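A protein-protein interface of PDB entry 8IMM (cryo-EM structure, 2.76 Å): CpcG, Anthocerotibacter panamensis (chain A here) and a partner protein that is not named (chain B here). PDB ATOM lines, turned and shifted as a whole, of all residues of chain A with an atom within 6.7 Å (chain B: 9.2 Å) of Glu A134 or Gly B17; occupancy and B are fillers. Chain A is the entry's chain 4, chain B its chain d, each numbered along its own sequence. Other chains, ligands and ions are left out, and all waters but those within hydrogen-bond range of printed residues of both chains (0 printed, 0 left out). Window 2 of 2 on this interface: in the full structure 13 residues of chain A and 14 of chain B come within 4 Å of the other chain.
The backbone carbonyl oxygen (O) of Lys A135 lies close to the backbone carbonyl oxygen (O) of Ser B15 (3.2 Å).
OG of Ser B15 sits at hydrogen-bond distance from O of Ala B11 (2.8 Å).
OE1 of Gln B16 lies close to O of Thr B12 (2.6 Å).
The side-chain sulfur (SD) of Met A1 sits close to the side-chain amino group (NZ) of Lys A135 (3.2 Å).
Among the printed residues, merely in contact across the chains: Glu A134 with Gly B17 (3.9 Å), Lys A135 with Gln B16 (3.4 Å), Lys A135 with Gly B17 (3.8 Å), Gly A136 with Asp B14 (3.4 Å), Gly A136 with Ser B15 (3.2 Å) and Tyr A137 with Ser B15 (3.3 Å).
Of chain B, only Gly B17 comes within 4 Å of Glu A134.
Gly B17 touches two residues of chain A.
No residue of chain B comes within 4 Å of Ala A133.
Of chain B, only Ser B15 (3.2 Å), Gln B16 (3.4 Å) and Gly B17 (3.8 Å) come within 4 Å of Lys A135.
Of the printed residues of chain A, Ser B15 touches Lys A135 (3.2 Å), Gly A136 (3.2 Å) and Tyr A137 (3.3 Å).
Of the printed residues of chain B, Tyr A137 touches Ser B15 (3.3 Å).
Ser A129 touches none of the printed residues of chain B.
Val B9 touches none of the printed residues of chain A.
The nearest residue of chain B that does not touch Glu A134 is Gln B16 (5.0 Å).
Of the 12 printed residues of chain A, 4 touch a printed residue of chain B.
Printed residues of chain A that touch a printed residue of chain B: Glu A134, Lys A135, Gly A136 and Tyr A137.
Hydrophobic or aromatic side chains of chain A within 4 Å of the printed part of chain B: Tyr A137.
Of the 12 printed residues of chain B, 4 touch a printed residue of chain A.
Among the printed residues, 7 pairs touch across the chains.
Among the printed residues, no Asp or Glu carboxylate lies within 4 Å of a Lys or Arg side-chain nitrogen of the other chain.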
ATOM      1  N   MET A   1     -27.663  -1.383   2.638  1.00  0.00           N
ATOM      2  CA  MET A   1     -28.592  -0.318   2.992  1.00  0.00           C
ATOM      3  C   MET A   1     -29.380  -0.743   4.226  1.00  0.00           C
ATOM      4  O   MET A   1     -28.803  -0.956   5.288  1.00  0.00           O
ATOM      5  CB  MET A   1     -29.515  -0.004   1.811  1.00  0.00           C
ATOM      6  CG  MET A   1     -30.356   1.265   1.933  1.00  0.00           C
ATOM      7  SD  MET A   1     -29.413   2.770   2.254  1.00  0.00           S
ATOM      8  CE  MET A   1     -30.169   3.330   3.778  1.00  0.00           C
ATOM      9  N   GLY A   2     -30.681  -0.886   4.088  1.00  0.00           N
ATOM     10  CA  GLY A   2     -31.515  -1.288   5.193  1.00  0.00           C
ATOM     11  C   GLY A   2     -32.835  -0.532   5.154  1.00  0.00           C
ATOM     12  O   GLY A   2     -33.559  -0.582   4.158  1.00  0.00           O
ATOM     13  N   LEU A   3     -33.129   0.148   6.257  1.00  0.00           N
ATOM     14  CA  LEU A   3     -34.337   0.939   6.350  1.00  0.00           C
ATOM     15  C   LEU A   3     -34.180   2.242   5.579  1.00  0.00           C
ATOM     16  O   LEU A   3     -33.065   2.717   5.361  1.00  0.00           O
ATOM     17  CB  LEU A   3     -34.664   1.246   7.806  1.00  0.00           C
ATOM     18  CG  LEU A   3     -35.090   0.090   8.694  1.00  0.00           C
ATOM     19  CD1 LEU A   3     -35.204   0.563  10.123  1.00  0.00           C
ATOM     20  CD2 LEU A   3     -36.396  -0.445   8.202  1.00  0.00           C
ATOM     21  N   SER A 129     -27.117  10.319  11.326  1.00  0.00           N
ATOM     22  CA  SER A 129     -26.232   9.585  12.216  1.00  0.00           C
ATOM     23  C   SER A 129     -26.518   8.098  12.238  1.00  0.00           C
ATOM     24  O   SER A 129     -25.654   7.321  12.650  1.00  0.00           O
ATOM     25  CB  SER A 129     -26.348  10.135  13.627  1.00  0.00           C
ATOM     26  OG  SER A 129     -27.502   9.623  14.252  1.00  0.00           O
ATOM     27  N   ILE A 130     -27.710   7.676  11.827  1.00  0.00           N
ATOM     28  CA  ILE A 130     -27.997   6.252  11.856  1.00  0.00           C
ATOM     29  C   ILE A 130     -27.191   5.520  10.800  1.00  0.00           C
ATOM     30  O   ILE A 130     -26.879   4.334  10.963  1.00  0.00           O
ATOM     31  CB  ILE A 130     -29.499   5.993  11.701  1.00  0.00           C
ATOM     32  CG1 ILE A 130     -29.793   4.546  12.058  1.00  0.00           C
ATOM     33  CG2 ILE A 130     -29.945   6.294  10.295  1.00  0.00           C
ATOM     34  CD1 ILE A 130     -29.408   4.183  13.458  1.00  0.00           C
ATOM     35  N   ILE A 131     -26.814   6.200   9.719  1.00  0.00           N
ATOM     36  CA  ILE A 131     -25.948   5.562   8.737  1.00  0.00           C
ATOM     37  C   ILE A 131     -24.612   5.224   9.370  1.00  0.00           C
ATOM     38  O   ILE A 131     -24.096   4.121   9.198  1.00  0.00           O
ATOM     39  CB  ILE A 131     -25.779   6.450   7.497  1.00  0.00           C
ATOM     40  CG1 ILE A 131     -27.137   6.820   6.932  1.00  0.00           C
ATOM     41  CG2 ILE A 131     -25.025   5.704   6.446  1.00  0.00           C
ATOM     42  CD1 ILE A 131     -27.061   7.596   5.664  1.00  0.00           C
ATOM     43  N   ILE A 132     -24.042   6.157  10.131  1.00  0.00           N
ATOM     44  CA  ILE A 132     -22.849   5.844  10.906  1.00  0.00           C
ATOM     45  C   ILE A 132     -23.127   4.688  11.845  1.00  0.00           C
ATOM     46  O   ILE A 132     -22.504   3.630  11.738  1.00  0.00           O
ATOM     47  CB  ILE A 132     -22.371   7.076  11.685  1.00  0.00           C
ATOM     48  CG1 ILE A 132     -22.139   8.243  10.749  1.00  0.00           C
ATOM     49  CG2 ILE A 132     -21.110   6.768  12.427  1.00  0.00           C
ATOM     50  CD1 ILE A 132     -22.062   9.522  11.470  1.00  0.00           C
ATOM     51  N   ALA A 133     -24.135   4.837  12.702  1.00  0.00           N
ATOM     52  CA  ALA A 133     -24.386   3.872  13.765  1.00  0.00           C
ATOM     53  C   ALA A 133     -24.546   2.463  13.225  1.00  0.00           C
ATOM     54  O   ALA A 133     -24.186   1.493  13.896  1.00  0.00           O
ATOM     55  CB  ALA A 133     -25.631   4.278  14.541  1.00  0.00           C
ATOM     56  N   GLU A 134     -25.071   2.323  12.014  1.00  0.00           N
ATOM     57  CA  GLU A 134     -25.416   1.014  11.493  1.00  0.00           C
ATOM     58  C   GLU A 134     -24.473   0.503  10.418  1.00  0.00           C
ATOM     59  O   GLU A 134     -24.485  -0.695  10.141  1.00  0.00           O
ATOM     60  CB  GLU A 134     -26.845   1.037  10.942  1.00  0.00           C
ATOM     61  CG  GLU A 134     -27.557  -0.295  11.018  1.00  0.00           C
ATOM     62  CD  GLU A 134     -27.395  -1.133   9.766  1.00  0.00           C
ATOM     63  OE1 GLU A 134     -27.333  -0.549   8.666  1.00  0.00           O
ATOM     64  OE2 GLU A 134     -27.320  -2.378   9.882  1.00  0.00           O
ATOM     65  N   LYS A 135     -23.647   1.358   9.804  1.00  0.00           N
ATOM     66  CA  LYS A 135     -22.811   0.919   8.697  1.00  0.00           C
ATOM     67  C   LYS A 135     -21.397   1.480   8.719  1.00  0.00           C
ATOM     68  O   LYS A 135     -20.589   1.090   7.873  1.00  0.00           O
ATOM     69  CB  LYS A 135     -23.448   1.298   7.362  1.00  0.00           C
ATOM     70  CG  LYS A 135     -24.863   0.855   7.165  1.00  0.00           C
ATOM     71  CD  LYS A 135     -25.397   1.470   5.905  1.00  0.00           C
ATOM     72  CE  LYS A 135     -26.897   1.402   5.854  1.00  0.00           C
ATOM     73  NZ  LYS A 135     -27.397   2.160   4.684  1.00  0.00           N
ATOM     74  N   GLY A 136     -21.066   2.376   9.634  1.00  0.00           N
ATOM     75  CA  GLY A 136     -19.748   2.961   9.661  1.00  0.00           C
ATOM     76  C   GLY A 136     -19.669   4.287   8.929  1.00  0.00           C
ATOM     77  O   GLY A 136     -20.411   4.575   7.985  1.00  0.00           O
ATOM     78  N   TYR A 137     -18.728   5.112   9.374  1.00  0.00           N
ATOM     79  CA  TYR A 137     -18.551   6.399   8.732  1.00  0.00           C
ATOM     80  C   TYR A 137     -18.068   6.241   7.302  1.00  0.00           C
ATOM     81  O   TYR A 137     -18.208   7.174   6.513  1.00  0.00           O
ATOM     82  CB  TYR A 137     -17.579   7.271   9.528  1.00  0.00           C
ATOM     83  CG  TYR A 137     -16.126   6.994   9.280  1.00  0.00           C
ATOM     84  CD1 TYR A 137     -15.492   5.925   9.863  1.00  0.00           C
ATOM     85  CD2 TYR A 137     -15.377   7.846   8.492  1.00  0.00           C
ATOM     86  CE1 TYR A 137     -14.167   5.684   9.630  1.00  0.00           C
ATOM     87  CE2 TYR A 137     -14.058   7.618   8.263  1.00  0.00           C
ATOM     88  CZ  TYR A 137     -13.454   6.539   8.835  1.00  0.00           C
ATOM     89  OH  TYR A 137     -12.120   6.309   8.601  1.00  0.00           O
ATOM     90  N   VAL B   9      -8.410  -3.237  15.560  1.00  0.00           N
ATOM     91  CA  VAL B   9      -9.485  -4.208  15.391  1.00  0.00           C
ATOM     92  C   VAL B   9     -10.844  -3.546  15.548  1.00  0.00           C
ATOM     93  O   VAL B   9     -11.734  -3.696  14.704  1.00  0.00           O
ATOM     94  CB  VAL B   9      -9.296  -5.350  16.399  1.00  0.00           C
ATOM     95  CG1 VAL B   9     -10.539  -6.153  16.534  1.00  0.00           C
ATOM     96  CG2 VAL B   9      -8.153  -6.225  15.962  1.00  0.00           C
ATOM     97  N   ILE B  10     -11.020  -2.794  16.629  1.00  0.00           N
ATOM     98  CA  ILE B  10     -12.320  -2.215  16.936  1.00  0.00           C
ATOM     99  C   ILE B  10     -12.690  -1.153  15.914  1.00  0.00           C
ATOM    100  O   ILE B  10     -13.838  -1.076  15.470  1.00  0.00           O
ATOM    101  CB  ILE B  10     -12.319  -1.666  18.369  1.00  0.00           C
ATOM    102  CG1 ILE B  10     -12.302  -2.821  19.360  1.00  0.00           C
ATOM    103  CG2 ILE B  10     -13.513  -0.784  18.603  1.00  0.00           C
ATOM    104  CD1 ILE B  10     -12.226  -2.378  20.775  1.00  0.00           C
ATOM    105  N   ALA B  11     -11.728  -0.320  15.518  1.00  0.00           N
ATOM    106  CA  ALA B  11     -11.991   0.708  14.523  1.00  0.00           C
ATOM    107  C   ALA B  11     -12.331   0.101  13.172  1.00  0.00           C
ATOM    108  O   ALA B  11     -13.241   0.573  12.486  1.00  0.00           O
ATOM    109  CB  ALA B  11     -10.786   1.629  14.405  1.00  0.00           C
ATOM    110  N   THR B  12     -11.611  -0.943  12.768  1.00  0.00           N
ATOM    111  CA  THR B  12     -11.915  -1.593  11.501  1.00  0.00           C
ATOM    112  C   THR B  12     -13.286  -2.246  11.530  1.00  0.00           C
ATOM    113  O   THR B  12     -14.018  -2.200  10.538  1.00  0.00           O
ATOM    114  CB  THR B  12     -10.844  -2.624  11.176  1.00  0.00           C
ATOM    115  OG1 THR B  12      -9.554  -2.045  11.392  1.00  0.00           O
ATOM    116  CG2 THR B  12     -10.961  -3.059   9.734  1.00  0.00           C
ATOM    117  N   ALA B  13     -13.654  -2.866  12.647  1.00  0.00           N
ATOM    118  CA  ALA B  13     -14.994  -3.427  12.754  1.00  0.00           C
ATOM    119  C   ALA B  13     -16.051  -2.335  12.720  1.00  0.00           C
ATOM    120  O   ALA B  13     -17.096  -2.492  12.083  1.00  0.00           O
ATOM    121  CB  ALA B  13     -15.114  -4.245  14.033  1.00  0.00           C
ATOM    122  N   ASP B  14     -15.793  -1.218  13.395  1.00  0.00           N
ATOM    123  CA  ASP B  14     -16.781  -0.160  13.534  1.00  0.00           C
ATOM    124  C   ASP B  14     -16.967   0.631  12.251  1.00  0.00           C
ATOM    125  O   ASP B  14     -18.051   1.169  12.014  1.00  0.00           O
ATOM    126  CB  ASP B  14     -16.375   0.773  14.671  1.00  0.00           C
ATOM    127  CG  ASP B  14     -17.362   1.887  14.888  1.00  0.00           C
ATOM    128  OD1 ASP B  14     -17.233   2.937  14.225  1.00  0.00           O
ATOM    129  OD2 ASP B  14     -18.274   1.721  15.722  1.00  0.00           O
ATOM    130  N   SER B  15     -15.936   0.718  11.418  1.00  0.00           N
ATOM    131  CA  SER B  15     -16.056   1.478  10.183  1.00  0.00           C
ATOM    132  C   SER B  15     -16.880   0.736   9.144  1.00  0.00           C
ATOM    133  O   SER B  15     -17.421   1.359   8.229  1.00  0.00           O
ATOM    134  CB  SER B  15     -14.672   1.798   9.643  1.00  0.00           C
ATOM    135  OG  SER B  15     -13.923   2.507  10.610  1.00  0.00           O
ATOM    136  N   GLN B  16     -16.955  -0.586   9.245  1.00  0.00           N
ATOM    137  CA  GLN B  16     -17.901  -1.371   8.467  1.00  0.00           C
ATOM    138  C   GLN B  16     -19.158  -1.730   9.240  1.00  0.00           C
ATOM    139  O   GLN B  16     -20.016  -2.429   8.697  1.00  0.00           O
ATOM    140  CB  GLN B  16     -17.246  -2.651   7.950  1.00  0.00           C
ATOM    141  CG  GLN B  16     -16.347  -2.465   6.760  1.00  0.00           C
ATOM    142  CD  GLN B  16     -14.913  -2.267   7.143  1.00  0.00           C
ATOM    143  OE1 GLN B  16     -14.614  -1.572   8.106  1.00  0.00           O
ATOM    144  NE2 GLN B  16     -14.007  -2.891   6.401  1.00  0.00           N
ATOM    145  N   GLY B  17     -19.287  -1.286  10.483  1.00  0.00           N
ATOM    146  CA  GLY B  17     -20.498  -1.525  11.234  1.00  0.00           C
ATOM    147  C   GLY B  17     -20.800  -2.991  11.425  1.00  0.00           C
ATOM    148  O   GLY B  17     -21.943  -3.418  11.258  1.00  0.00           O
ATOM    149  N   ARG B  18     -19.789  -3.773  11.773  1.00  0.00           N
ATOM    150  CA  ARG B  18     -19.936  -5.208  11.913  1.00  0.00           C
ATOM    151  C   ARG B  18     -19.378  -5.655  13.251  1.00  0.00           C
ATOM    152  O   ARG B  18     -18.570  -4.969  13.876  1.00  0.00           O
ATOM    153  CB  ARG B  18     -19.229  -5.955  10.786  1.00  0.00           C
ATOM    154  CG  ARG B  18     -17.730  -5.888  10.855  1.00  0.00           C
ATOM    155  CD  ARG B  18     -17.110  -6.259   9.532  1.00  0.00           C
ATOM    156  NE  ARG B  18     -15.685  -5.956   9.504  1.00  0.00           N
ATOM    157  CZ  ARG B  18     -14.763  -6.636  10.173  1.00  0.00           C
ATOM    158  NH1 ARG B  18     -15.109  -7.675  10.918  1.00  0.00           N
ATOM    159  NH2 ARG B  18     -13.491  -6.284  10.091  1.00  0.00           N
ATOM    160  N   PHE B  19     -19.827  -6.822  13.685  1.00  0.00           N
ATOM    161  CA  PHE B  19     -19.320  -7.419  14.906  1.00  0.00           C
ATOM    162  C   PHE B  19     -17.889  -7.894  14.690  1.00  0.00           C
ATOM    163  O   PHE B  19     -17.427  -8.047  13.559  1.00  0.00           O
ATOM    164  CB  PHE B  19     -20.198  -8.594  15.307  1.00  0.00           C
ATOM    165  CG  PHE B  19     -21.448  -8.205  16.029  1.00  0.00           C
ATOM    166  CD1 PHE B  19     -21.477  -8.114  17.398  1.00  0.00           C
ATOM    167  CD2 PHE B  19     -22.601  -7.950  15.329  1.00  0.00           C
ATOM    168  CE1 PHE B  19     -22.629  -7.777  18.044  1.00  0.00           C
ATOM    169  CE2 PHE B  19     -23.747  -7.605  15.975  1.00  0.00           C
ATOM    170  CZ  PHE B  19     -23.763  -7.522  17.329  1.00  0.00           C
ATOM    171  N   LEU B  20     -17.181  -8.128  15.786  1.00  0.00           N
ATOM    172  CA  LEU B  20     -15.826  -8.652  15.691  1.00  0.00           C
ATOM    173  C   LEU B  20     -15.869 -10.109  15.256  1.00  0.00           C
ATOM    174  O   LEU B  20     -16.399 -10.962  15.974  1.00  0.00           O
ATOM    175  CB  LEU B  20     -15.113  -8.525  17.032  1.00  0.00           C
ATOM    176  CG  LEU B  20     -15.041  -7.134  17.642  1.00  0.00           C
ATOM    177  CD1 LEU B  20     -14.662  -7.237  19.095  1.00  0.00           C
ATOM    178  CD2 LEU B  20     -14.048  -6.303  16.901  1.00  0.00           C
